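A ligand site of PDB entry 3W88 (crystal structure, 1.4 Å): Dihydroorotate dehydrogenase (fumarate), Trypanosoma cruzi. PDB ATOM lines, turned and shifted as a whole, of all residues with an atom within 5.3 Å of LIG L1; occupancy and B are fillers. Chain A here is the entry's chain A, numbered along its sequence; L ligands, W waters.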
ATOM      1  N   ALA A  20     -22.584  -0.320  35.385  1.00  0.00           N
ATOM      2  CA  ALA A  20     -22.525  -0.591  33.949  1.00  0.00           C
ATOM      3  C   ALA A  20     -21.251  -1.410  33.674  1.00  0.00           C
ATOM      4  O   ALA A  20     -20.183  -1.157  34.218  1.00  0.00           O
ATOM      5  CB  ALA A  20     -22.476   0.737  33.190  1.00  0.00           C
ATOM      6  N   ALA A  21     -21.343  -2.345  32.716  1.00  0.00           N
ATOM      7  CA  ALA A  21     -20.168  -3.089  32.332  1.00  0.00           C
ATOM      8  C   ALA A  21     -19.023  -2.198  31.941  1.00  0.00           C
ATOM      9  O   ALA A  21     -19.196  -1.185  31.270  1.00  0.00           O
ATOM     10  CB  ALA A  21     -20.534  -4.046  31.229  1.00  0.00           C
ATOM     11  N   GLY A  22     -17.834  -2.590  32.364  1.00  0.00           N
ATOM     12  CA  GLY A  22     -16.640  -1.845  32.181  1.00  0.00           C
ATOM     13  C   GLY A  22     -16.251  -0.925  33.262  1.00  0.00           C
ATOM     14  O   GLY A  22     -15.058  -0.531  33.346  1.00  0.00           O
ATOM     15  N   VAL A  23     -17.182  -0.488  34.124  1.00  0.00           N
ATOM     16  CA  VAL A  23     -16.871   0.421  35.238  1.00  0.00           C
ATOM     17  C   VAL A  23     -16.775  -0.285  36.552  1.00  0.00           C
ATOM     18  O   VAL A  23     -17.689  -1.025  36.867  1.00  0.00           O
ATOM     19  CB  VAL A  23     -17.902   1.603  35.269  1.00  0.00           C
ATOM     20  CG1 VAL A  23     -17.647   2.521  36.450  1.00  0.00           C
ATOM     21  CG2 VAL A  23     -17.897   2.376  33.961  1.00  0.00           C
ATOM     22  N   LYS A  45     -16.448  -6.721  33.715  1.00  0.00           N
ATOM     23  CA  LYS A  45     -15.913  -6.118  32.488  1.00  0.00           C
ATOM     24  C   LYS A  45     -16.120  -7.055  31.303  1.00  0.00           C
ATOM     25  O   LYS A  45     -15.866  -8.246  31.444  1.00  0.00           O
ATOM     26  CB  LYS A  45     -14.418  -5.906  32.669  1.00  0.00           C
ATOM     27  CG  LYS A  45     -13.663  -5.441  31.442  1.00  0.00           C
ATOM     28  CD  LYS A  45     -14.063  -4.120  30.862  1.00  0.00           C
ATOM     29  CE  LYS A  45     -13.584  -3.821  29.498  1.00  0.00           C
ATOM     30  NZ  LYS A  45     -13.984  -2.438  29.025  1.00  0.00           N
ATOM     31  N   SER A  46     -16.530  -6.560  30.185  1.00  0.00           N
ATOM     32  CA  SER A  46     -16.647  -7.449  29.025  1.00  0.00           C
ATOM     33  C   SER A  46     -15.294  -8.154  28.744  1.00  0.00           C
ATOM     34  O   SER A  46     -14.264  -7.509  28.730  1.00  0.00           O
ATOM     35  CB  SER A  46     -17.014  -6.696  27.775  1.00  0.00           C
ATOM     36  OG  SER A  46     -18.328  -6.168  27.858  1.00  0.00           O
ATOM     37  N   TYR A  60      -9.657   7.268  28.554  1.00  0.00           N
ATOM     38  CA  TYR A  60     -10.892   7.670  29.191  1.00  0.00           C
ATOM     39  C   TYR A  60     -10.712   9.070  29.697  1.00  0.00           C
ATOM     40  O   TYR A  60      -9.760   9.308  30.339  1.00  0.00           O
ATOM     41  CB  TYR A  60     -11.260   6.741  30.366  1.00  0.00           C
ATOM     42  CG  TYR A  60     -12.430   7.246  31.240  1.00  0.00           C
ATOM     43  CD1 TYR A  60     -13.732   6.963  30.906  1.00  0.00           C
ATOM     44  CD2 TYR A  60     -12.224   8.022  32.341  1.00  0.00           C
ATOM     45  CE1 TYR A  60     -14.781   7.427  31.706  1.00  0.00           C
ATOM     46  CE2 TYR A  60     -13.267   8.485  33.113  1.00  0.00           C
ATOM     47  CZ  TYR A  60     -14.530   8.187  32.774  1.00  0.00           C
ATOM     48  OH  TYR A  60     -15.485   8.661  33.565  1.00  0.00           O
ATOM     49  N   SER A  67     -18.558  11.577  29.680  1.00  0.00           N
ATOM     50  CA  SER A  67     -17.274  10.941  29.440  1.00  0.00           C
ATOM     51  C   SER A  67     -17.135  10.488  28.010  1.00  0.00           C
ATOM     52  O   SER A  67     -18.078  10.365  27.287  1.00  0.00           O
ATOM     53  CB  SER A  67     -17.092   9.718  30.384  1.00  0.00           C
ATOM     54  OG  SER A  67     -17.958   8.679  29.999  1.00  0.00           O
ATOM     55  N   ASN A  69     -14.580   7.511  25.931  1.00  0.00           N
ATOM     56  CA  ASN A  69     -13.625   6.407  26.085  1.00  0.00           C
ATOM     57  C   ASN A  69     -13.422   5.646  24.804  1.00  0.00           C
ATOM     58  O   ASN A  69     -14.289   5.409  23.984  1.00  0.00           O
ATOM     59  CB  ASN A  69     -14.027   5.418  27.210  1.00  0.00           C
ATOM     60  CG  ASN A  69     -14.921   4.319  26.747  1.00  0.00           C
ATOM     61  OD1 ASN A  69     -14.498   3.265  26.221  1.00  0.00           O
ATOM     62  ND2 ASN A  69     -16.245   4.452  26.907  1.00  0.00           N
ATOM     63  N   MET A  71     -11.413   2.405  25.347  1.00  0.00           N
ATOM     64  CA  MET A  71     -10.568   1.593  26.217  1.00  0.00           C
ATOM     65  C   MET A  71      -9.899   0.564  25.374  1.00  0.00           C
ATOM     66  O   MET A  71      -8.754   0.173  25.802  1.00  0.00           O
ATOM     67  CB  MET A  71     -11.411   0.952  27.276  1.00  0.00           C
ATOM     68  CG  MET A  71     -12.180   1.878  28.186  1.00  0.00           C
ATOM     69  SD  MET A  71     -11.194   3.115  29.028  1.00  0.00           S
ATOM     70  CE  MET A  71     -10.416   2.201  30.218  1.00  0.00           C
ATOM     71  N   LEU A  73     -11.160  -2.689  25.081  1.00  0.00           N
ATOM     72  CA  LEU A  73     -11.446  -3.961  25.672  1.00  0.00           C
ATOM     73  C   LEU A  73     -10.268  -4.474  26.521  1.00  0.00           C
ATOM     74  O   LEU A  73     -10.000  -5.725  26.443  1.00  0.00           O
ATOM     75  CB  LEU A  73     -11.953  -4.909  24.581  1.00  0.00           C
ATOM     76  CG  LEU A  73     -12.737  -6.131  24.882  1.00  0.00           C
ATOM     77  CD1 LEU A  73     -13.873  -6.017  25.988  1.00  0.00           C
ATOM     78  CD2 LEU A  73     -13.406  -6.569  23.552  1.00  0.00           C
ATOM     79  N   SER A  99     -20.265 -10.272  31.587  1.00  0.00           N
ATOM     80  CA  SER A  99     -20.309  -9.711  30.222  1.00  0.00           C
ATOM     81  C   SER A  99     -19.221 -10.344  29.340  1.00  0.00           C
ATOM     82  O   SER A  99     -18.057 -10.433  29.679  1.00  0.00           O
ATOM     83  CB  SER A  99     -20.105  -8.190  30.246  1.00  0.00           C
ATOM     84  OG  SER A  99     -20.153  -7.683  28.902  1.00  0.00           O
ATOM     85  N   GLU A 127     -24.555 -11.390  30.204  1.00  0.00           N
ATOM     86  CA  GLU A 127     -24.855 -10.222  29.394  1.00  0.00           C
ATOM     87  C   GLU A 127     -23.916 -10.246  28.194  1.00  0.00           C
ATOM     88  O   GLU A 127     -22.729 -10.098  28.259  1.00  0.00           O
ATOM     89  CB  GLU A 127     -24.744  -8.885  30.241  1.00  0.00           C
ATOM     90  CG  GLU A 127     -25.121  -7.631  29.391  1.00  0.00           C
ATOM     91  CD  GLU A 127     -25.054  -6.337  30.215  1.00  0.00           C
ATOM     92  OE1 GLU A 127     -23.968  -5.746  30.243  1.00  0.00           O
ATOM     93  OE2 GLU A 127     -26.121  -5.935  30.787  1.00  0.00           O
ATOM     94  N   ASN A 129     -22.340  -8.786  25.013  1.00  0.00           N
ATOM     95  CA  ASN A 129     -22.114  -7.442  24.473  1.00  0.00           C
ATOM     96  C   ASN A 129     -22.106  -7.452  22.942  1.00  0.00           C
ATOM     97  O   ASN A 129     -21.229  -7.911  22.379  1.00  0.00           O
ATOM     98  CB  ASN A 129     -20.771  -6.937  25.022  1.00  0.00           C
ATOM     99  CG  ASN A 129     -20.482  -5.500  24.660  1.00  0.00           C
ATOM    100  OD1 ASN A 129     -21.152  -4.929  23.905  1.00  0.00           O
ATOM    101  ND2 ASN A 129     -19.403  -5.004  25.145  1.00  0.00           N
ATOM    102  N   LYS A 166     -26.485  -6.603  25.562  1.00  0.00           N
ATOM    103  CA  LYS A 166     -26.158  -5.175  25.708  1.00  0.00           C
ATOM    104  C   LYS A 166     -26.158  -4.590  24.287  1.00  0.00           C
ATOM    105  O   LYS A 166     -25.357  -4.993  23.425  1.00  0.00           O
ATOM    106  CB  LYS A 166     -24.806  -5.036  26.345  1.00  0.00           C
ATOM    107  CG  LYS A 166     -24.290  -3.584  26.524  1.00  0.00           C
ATOM    108  CD  LYS A 166     -25.015  -2.861  27.613  1.00  0.00           C
ATOM    109  CE  LYS A 166     -24.329  -1.530  27.947  1.00  0.00           C
ATOM    110  NZ  LYS A 166     -23.123  -1.699  28.695  1.00  0.00           N
ATOM    111  N   VAL A 195     -28.467   1.530  27.216  1.00  0.00           N
ATOM    112  CA  VAL A 195     -27.618   1.425  26.033  1.00  0.00           C
ATOM    113  C   VAL A 195     -26.149   1.393  26.387  1.00  0.00           C
ATOM    114  O   VAL A 195     -25.753   1.839  27.478  1.00  0.00           O
ATOM    115  CB  VAL A 195     -27.852   2.623  25.079  1.00  0.00           C
ATOM    116  CG1 VAL A 195     -29.263   2.588  24.492  1.00  0.00           C
ATOM    117  CG2 VAL A 195     -27.603   3.973  25.730  1.00  0.00           C
ATOM    118  N   ASN A 196     -25.341   0.886  25.457  1.00  0.00           N
ATOM    119  CA  ASN A 196     -23.905   1.134  25.422  1.00  0.00           C
ATOM    120  C   ASN A 196     -23.646   2.619  25.089  1.00  0.00           C
ATOM    121  O   ASN A 196     -24.571   3.421  24.853  1.00  0.00           O
ATOM    122  CB  ASN A 196     -23.252   0.184  24.401  1.00  0.00           C
ATOM    123  CG  ASN A 196     -21.903  -0.257  24.859  1.00  0.00           C
ATOM    124  OD1 ASN A 196     -21.054   0.546  25.245  1.00  0.00           O
ATOM    125  ND2 ASN A 196     -21.654  -1.544  24.748  1.00  0.00           N
ATOM    126  N   SER A 197     -22.375   2.980  25.111  1.00  0.00           N
ATOM    127  CA  SER A 197     -22.013   4.363  24.817  1.00  0.00           C
ATOM    128  C   SER A 197     -22.468   4.770  23.445  1.00  0.00           C
ATOM    129  O   SER A 197     -22.632   4.005  22.520  1.00  0.00           O
ATOM    130  CB  SER A 197     -20.491   4.541  25.012  1.00  0.00           C
ATOM    131  OG  SER A 197     -19.717   3.647  24.385  1.00  0.00           O
ATOM    132  N   LEU A 222     -19.396   7.958  23.979  1.00  0.00           N
ATOM    133  CA  LEU A 222     -19.864   8.908  24.960  1.00  0.00           C
ATOM    134  C   LEU A 222     -20.826   8.261  26.001  1.00  0.00           C
ATOM    135  O   LEU A 222     -21.720   7.517  25.677  1.00  0.00           O
ATOM    136  CB  LEU A 222     -20.616  10.030  24.271  1.00  0.00           C
ATOM    137  CG  LEU A 222     -19.890  10.751  23.141  1.00  0.00           C
ATOM    138  CD1 LEU A 222     -20.852  11.673  22.447  1.00  0.00           C
ATOM    139  CD2 LEU A 222     -18.720  11.488  23.692  1.00  0.00           C
ATOM    140  N   GLY A 223     -20.608   8.721  27.227  1.00  0.00           N
ATOM    141  CA  GLY A 223     -21.502   8.426  28.291  1.00  0.00           C
ATOM    142  C   GLY A 223     -21.867   9.598  29.110  1.00  0.00           C
ATOM    143  O   GLY A 223     -21.228  10.685  28.924  1.00  0.00           O
ATOM    144  N   GLY A 224     -22.772   9.478  30.096  1.00  0.00           N
ATOM    145  CA  GLY A 224     -23.077  10.523  31.009  1.00  0.00           C
ATOM    146  C   GLY A 224     -24.239  11.404  30.598  1.00  0.00           C
ATOM    147  O   GLY A 224     -25.167  10.934  29.878  1.00  0.00           O
ATOM    148  N   ILE A 227     -26.090  11.655  27.126  1.00  0.00           N
ATOM    149  CA  ILE A 227     -26.796  10.571  26.487  1.00  0.00           C
ATOM    150  C   ILE A 227     -28.080  10.148  27.151  1.00  0.00           C
ATOM    151  O   ILE A 227     -28.737   9.261  26.692  1.00  0.00           O
ATOM    152  CB  ILE A 227     -25.903   9.309  26.290  1.00  0.00           C
ATOM    153  CG1 ILE A 227     -25.708   8.469  27.563  1.00  0.00           C
ATOM    154  CG2 ILE A 227     -24.532   9.663  25.704  1.00  0.00           C
ATOM    155  CD1 ILE A 227     -25.203   7.104  27.255  1.00  0.00           C
ATOM    156  N   CYS A 250     -29.444   1.853  30.942  1.00  0.00           N
ATOM    157  CA  CYS A 250     -28.124   2.295  31.183  1.00  0.00           C
ATOM    158  C   CYS A 250     -27.927   3.570  30.356  1.00  0.00           C
ATOM    159  O   CYS A 250     -28.226   3.597  29.133  1.00  0.00           O
ATOM    160  CB  CYS A 250     -27.095   1.274  30.664  1.00  0.00           C
ATOM    161  SG  CYS A 250     -25.406   1.597  31.153  1.00  0.00           S
ATOM    162  N   GLY A 251     -27.427   4.644  30.965  1.00  0.00           N
ATOM    163  CA  GLY A 251     -27.056   5.831  30.235  1.00  0.00           C
ATOM    164  C   GLY A 251     -27.507   7.058  30.948  1.00  0.00           C
ATOM    165  O   GLY A 251     -28.708   7.291  31.176  1.00  0.00           O
ATOM    166  N   GLY A 252     -26.568   7.859  31.418  1.00  0.00           N
ATOM    167  CA  GLY A 252     -26.898   9.147  31.989  1.00  0.00           C
ATOM    168  C   GLY A 252     -27.461   9.177  33.336  1.00  0.00           C
ATOM    169  O   GLY A 252     -28.036  10.188  33.772  1.00  0.00           O
ATOM    170  N   VAL A 253     -27.301   8.109  34.113  1.00  0.00           N
ATOM    171  CA  VAL A 253     -27.811   8.102  35.501  1.00  0.00           C
ATOM    172  C   VAL A 253     -26.791   8.735  36.440  1.00  0.00           C
ATOM    173  O   VAL A 253     -25.718   8.164  36.675  1.00  0.00           O
ATOM    174  CB  VAL A 253     -28.140   6.673  35.955  1.00  0.00           C
ATOM    175  CG1 VAL A 253     -28.634   6.662  37.411  1.00  0.00           C
ATOM    176  CG2 VAL A 253     -29.248   6.070  35.068  1.00  0.00           C
ATOM    177  N   GLN A 271     -28.419   0.656  35.396  1.00  0.00           N
ATOM    178  CA  GLN A 271     -26.951   0.531  35.440  1.00  0.00           C
ATOM    179  C   GLN A 271     -26.332   1.917  35.433  1.00  0.00           C
ATOM    180  O   GLN A 271     -26.891   2.874  34.868  1.00  0.00           O
ATOM    181  CB  GLN A 271     -26.413  -0.244  34.261  1.00  0.00           C
ATOM    182  CG  GLN A 271     -27.154  -1.540  33.943  1.00  0.00           C
ATOM    183  CD  GLN A 271     -26.474  -2.381  32.940  1.00  0.00           C
ATOM    184  OE1 GLN A 271     -25.741  -1.884  32.069  1.00  0.00           O
ATOM    185  NE2 GLN A 271     -26.615  -3.692  33.057  1.00  0.00           N
ATOM    186  N   VAL A 272     -25.187   2.050  36.104  1.00  0.00           N
ATOM    187  CA  VAL A 272     -24.504   3.344  36.337  1.00  0.00           C
ATOM    188  C   VAL A 272     -23.066   3.217  35.868  1.00  0.00           C
ATOM    189  O   VAL A 272     -22.310   2.427  36.444  1.00  0.00           O
ATOM    190  CB  VAL A 272     -24.615   3.700  37.812  1.00  0.00           C
ATOM    191  CG1 VAL A 272     -24.079   5.138  37.974  1.00  0.00           C
ATOM    192  CG2 VAL A 272     -26.056   3.551  38.342  1.00  0.00           C
ATOM    193  N   GLY A 273     -22.687   3.980  34.844  1.00  0.00           N
ATOM    194  CA  GLY A 273     -21.373   3.930  34.282  1.00  0.00           C
ATOM    195  C   GLY A 273     -20.540   5.141  34.679  1.00  0.00           C
ATOM    196  O   GLY A 273     -19.913   5.195  35.754  1.00  0.00           O
ATOM    197  N   THR A 274     -20.587   6.184  33.839  1.00  0.00           N
ATOM    198  CA  THR A 274     -19.816   7.408  34.042  1.00  0.00           C
ATOM    199  C   THR A 274     -19.943   7.918  35.474  1.00  0.00           C
ATOM    200  O   THR A 274     -18.918   8.274  36.094  1.00  0.00           O
ATOM    201  CB  THR A 274     -20.217   8.484  33.031  1.00  0.00           C
ATOM    202  OG1 THR A 274     -19.977   7.991  31.717  1.00  0.00           O
ATOM    203  CG2 THR A 274     -19.487   9.753  33.253  1.00  0.00           C
ATOM    204  N   ALA A 275     -21.171   8.068  35.973  1.00  0.00           N
ATOM    205  CA  ALA A 275     -21.292   8.659  37.274  1.00  0.00           C
ATOM    206  C   ALA A 275     -20.600   7.868  38.379  1.00  0.00           C
ATOM    207  O   ALA A 275     -20.123   8.423  39.398  1.00  0.00           O
ATOM    208  CB  ALA A 275     -22.743   8.892  37.594  1.00  0.00           C
HETATM  209  N1  LIG L   1     -20.019  -1.433  28.015  1.00  0.00           N
HETATM  210  C1  LIG L   1     -19.932  -2.802  27.892  1.00  0.00           C
HETATM  211  O1  LIG L   1     -20.950  -3.434  27.633  1.00  0.00           O
HETATM  212  N2  LIG L   1     -18.755  -3.455  28.201  1.00  0.00           N
HETATM  213  C2  LIG L   1     -17.667  -2.857  28.577  1.00  0.00           C
HETATM  214  O2  LIG L   1     -16.597  -3.520  28.857  1.00  0.00           O
HETATM  215  C3  LIG L   1     -17.626  -1.436  28.662  1.00  0.00           C
HETATM  216  N3  LIG L   1     -16.594  -0.782  29.090  1.00  0.00           N
HETATM  217  C4  LIG L   1     -16.711   0.536  29.453  1.00  0.00           C
HETATM  218  C5  LIG L   1     -15.618   1.222  29.966  1.00  0.00           C
HETATM  219  C6  LIG L   1     -15.695   2.556  30.323  1.00  0.00           C
HETATM  220  C7  LIG L   1     -14.556   3.332  30.939  1.00  0.00           C
HETATM  221  C8  LIG L   1     -16.925   3.229  30.140  1.00  0.00           C
HETATM  222  C9  LIG L   1     -17.094   4.703  30.518  1.00  0.00           C
HETATM  223  C10 LIG L   1     -17.988   2.575  29.553  1.00  0.00           C
HETATM  224  C11 LIG L   1     -17.924   1.248  29.164  1.00  0.00           C
HETATM  225  N4  LIG L   1     -19.018   0.555  28.644  1.00  0.00           N
HETATM  226  C12 LIG L   1     -18.926  -0.825  28.435  1.00  0.00           C
HETATM  227  C13 LIG L   1     -20.294   1.219  28.407  1.00  0.00           C
HETATM  228  C14 LIG L   1     -21.061   1.398  29.700  1.00  0.00           C
HETATM  229  O3  LIG L   1     -21.427   0.089  30.187  1.00  0.00           O
HETATM  230  C15 LIG L   1     -22.334   2.149  29.505  1.00  0.00           C
HETATM  231  O4  LIG L   1     -23.141   1.452  28.526  1.00  0.00           O
HETATM  232  C16 LIG L   1     -22.110   3.591  28.999  1.00  0.00           C
HETATM  233  O5  LIG L   1     -20.949   4.206  29.622  1.00  0.00           O
HETATM  234  C17 LIG L   1     -23.311   4.500  29.208  1.00  0.00           C
HETATM  235  O6  LIG L   1     -23.682   4.584  30.574  1.00  0.00           O
HETATM  236  P1  LIG L   1     -23.301   5.948  31.398  1.00  0.00           P
HETATM  237  O7  LIG L   1     -23.787   5.636  32.775  1.00  0.00           O
HETATM  238  O8  LIG L   1     -23.984   7.088  30.724  1.00  0.00           O
HETATM  239  O9  LIG L   1     -21.784   6.067  31.362  1.00  0.00           O
HETATM  240  O1  LG2 L   2     -13.567   0.248  24.899  1.00  0.00           O
HETATM  241  C1  LG2 L   2     -14.181  -0.615  25.571  1.00  0.00           C
HETATM  242  O2  LG2 L   2     -13.655  -1.505  26.257  1.00  0.00           O
HETATM  243  C2  LG2 L   2     -15.634  -0.479  25.624  1.00  0.00           C
HETATM  244  N1  LG2 L   2     -16.109   0.856  25.750  1.00  0.00           N
HETATM  245  C3  LG2 L   2     -17.479   1.085  25.747  1.00  0.00           C
HETATM  246  O3  LG2 L   2     -17.881   2.261  25.899  1.00  0.00           O
HETATM  247  N2  LG2 L   2     -18.317   0.076  25.439  1.00  0.00           N
HETATM  248  C4  LG2 L   2     -17.900  -1.267  25.315  1.00  0.00           C
HETATM  249  O4  LG2 L   2     -18.779  -2.113  25.083  1.00  0.00           O
HETATM  250  C5  LG2 L   2     -16.509  -1.506  25.352  1.00  0.00           C
HETATM  251  C6  LG2 L   2     -16.054  -2.935  25.150  1.00  0.00           C
HETATM  252  C7  LG2 L   2     -16.215  -3.352  23.647  1.00  0.00           C
HETATM  253  C8  LG2 L   2     -15.320  -2.608  22.785  1.00  0.00           C
HETATM  254  C9  LG2 L   2     -14.998  -3.401  21.407  1.00  0.00           C
HETATM  255  C10 LG2 L   2     -13.714  -3.056  20.897  1.00  0.00           C
HETATM  256  C11 LG2 L   2     -13.418  -1.689  20.777  1.00  0.00           C
HETATM  257  C12 LG2 L   2     -12.195  -1.229  20.251  1.00  0.00           C
HETATM  258  C13 LG2 L   2     -11.959   0.189  20.146  1.00  0.00           C
HETATM  259  C14 LG2 L   2     -10.724   0.659  19.638  1.00  0.00           C
HETATM  260  C15 LG2 L   2      -9.742  -0.292  19.252  1.00  0.00           C
HETATM  261  C16 LG2 L   2      -8.517   0.175  18.734  1.00  0.00           C
HETATM  262  O5  LG2 L   2      -7.608  -0.643  18.373  1.00  0.00           O
HETATM  263  O6  LG2 L   2      -8.325   1.425  18.572  1.00  0.00           O
HETATM  264  C17 LG2 L   2      -9.999  -1.703  19.367  1.00  0.00           C
HETATM  265  C18 LG2 L   2     -11.224  -2.200  19.885  1.00  0.00           C
HETATM  266  C19 LG2 L   2     -11.521  -3.603  19.998  1.00  0.00           C
HETATM  267  C20 LG2 L   2     -12.782  -4.032  20.501  1.00  0.00           C
HETATM  268  O   HOH W   1     -21.988  -5.980  28.338  1.00  0.00           O
HETATM  269  O   HOH W   2     -13.002  -0.767  31.146  1.00  0.00           O
HETATM  270  O   HOH W   3     -26.331   5.302  33.534  1.00  0.00           O
HETATM  271  O   HOH W   4     -23.631   7.652  34.682  1.00  0.00           O
HETATM  272  O   HOH W   5     -19.688   5.444  27.752  1.00  0.00           O
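CB of Ala 20 touches O3 of LIG L1, at 3.2 Å.
Gly 22 touches LIG L1 (CA to N3, 3.3 Å).
CD1 of Tyr 60 touches C7 of LIG L1, at 3.7 Å.
Asn 69 touches LIG L1 (ND2 to C8, 3.5 Å).
Met 71 touches LIG L1 (SD to C7, 3.9 Å).
Asn 196 touches LIG L1.
Ser 197 touches LIG L1.
Gly 223 touches LIG L1.
Ile 227 touches LIG L1 (CD1 to O8, 3.7 Å).
CA of Gly 251 touches O8 of LIG L1 (3.4 Å).
Val 272 touches LIG L1 (C to O7, 3.99 Å).
Hydrophobic or aromatic side chains that line LIG L1: Ala 20, Ala 21, Tyr 60, Met 71 and Ile 227.
An oxygen (O4) of LG2 L2 sits close to a nitrogen (N2) of LIG L1 (3.4 Å).
The backbone NH of Gly 224 sits at hydrogen-bond distance from an oxygen (O8) of LIG L1, at 2.8 Å.
OG1 of Thr 274 lies within hydrogen-bond range of O9 of LIG L1 (2.7 Å).
N2 of LG2 L2 lies within hydrogen-bond range of OD1 of Asn 196, at 2.8 Å.
The backbone NH (N) of Gly 252 sits at hydrogen-bond distance from an oxygen (O8) of LIG L1 (2.8 Å).
N of Thr 274 sits at hydrogen-bond distance from O9 of LIG L1.
O4 of LG2 L2 sits at hydrogen-bond distance from ND2 of Asn 129.
An oxygen (O4) of LIG L1 lies within hydrogen-bond range of the side-chain sulfur (SG) of Cys 250, 3.5 Å away.
NZ of Lys 45 sits at hydrogen-bond distance from O2 of LIG L1 (2.8 Å).
The side-chain hydroxyl of Ser 197 lies within hydrogen-bond range of an oxygen (O3) of LG2 L2 (2.8 Å).
O of Ala 21 is in hydrogen-bond range of O3 of LIG L1, at 2.8 Å.
NZ of Lys 45 is in salt-bridge range of O2 of LG2 L2, 2.9 Å away.
N of Ser 46 sits at hydrogen-bond distance from O2 of LIG L1.
O1 of LG2 L2 lies within hydrogen-bond range of N of Met 71 (3.1 Å).
An oxygen (O7) of LIG L1 sits at hydrogen-bond distance from the backbone NH (N) of Gly 273 (2.9 Å).
The side-chain amide nitrogen of Asn 129 lies within hydrogen-bond range of an oxygen (O1) of LIG L1.
N2 of LIG L1 sits at hydrogen-bond distance from OG of Ser 46, at 2.8 Å.
The side-chain amino group (NZ) of Lys 166 is in hydrogen-bond range of an oxygen (O3) of LIG L1 (2.9 Å).
O4 of LIG L1 lies within hydrogen-bond range of O of Val 195 (2.8 Å).
The side-chain amide nitrogen (ND2) of Asn 69 sits at hydrogen-bond distance from an oxygen (O3) of LG2 L2.
The backbone NH (N) of Leu 73 sits at hydrogen-bond distance from an oxygen (O2) of LG2 L2 (3.0 Å).
The side-chain hydroxyl of Thr 274 lies within hydrogen-bond range of the side-chain hydroxyl of Ser 67 (2.7 Å).
N of Ala 20 sits at hydrogen-bond distance from O of Val 272, 3.0 Å away.
OG of Ser 46 is in hydrogen-bond range of ND2 of Asn 129.
The backbone carbonyl oxygen (O) of Cys 250 lies within hydrogen-bond range of the backbone NH (N) of Val 195 (2.8 Å).
The side-chain hydroxyl (OG) of Ser 197 is in hydrogen-bond range of the side-chain amide oxygen (OD1) of Asn 196 (3.5 Å).
The side-chain hydroxyl (OG) of Ser 46 is in hydrogen-bond range of the side-chain hydroxyl (OG) of Ser 99 (2.6 Å).
The backbone NH (N) of Ser 67 sits at hydrogen-bond distance from the backbone carbonyl oxygen (O) of Gly 223 (2.9 Å).
The backbone NH of Met 71 sits at hydrogen-bond distance from the side-chain amide oxygen of Asn 69 (3.3 Å).
Water W5 lies within hydrogen-bond range of an oxygen (O5) of LIG L1 and the backbone NH of Gly 223.
Water W4 lies within hydrogen-bond range of an oxygen (O7) of LIG L1 (2.8 Å), the backbone NH (N) of Ala 275 (2.8 Å), the backbone carbonyl oxygen (O) of Val 253 (2.9 Å) and the backbone NH (N) of Thr 274 (3.5 Å).
Water W1 lies within hydrogen-bond range of the side-chain hydroxyl of Ser 99, the side-chain carboxylate of Glu 127 and an oxygen (O1) of LIG L1.
Water W2 lies within hydrogen-bond range of NZ of Lys 45 and O of Gly 22.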
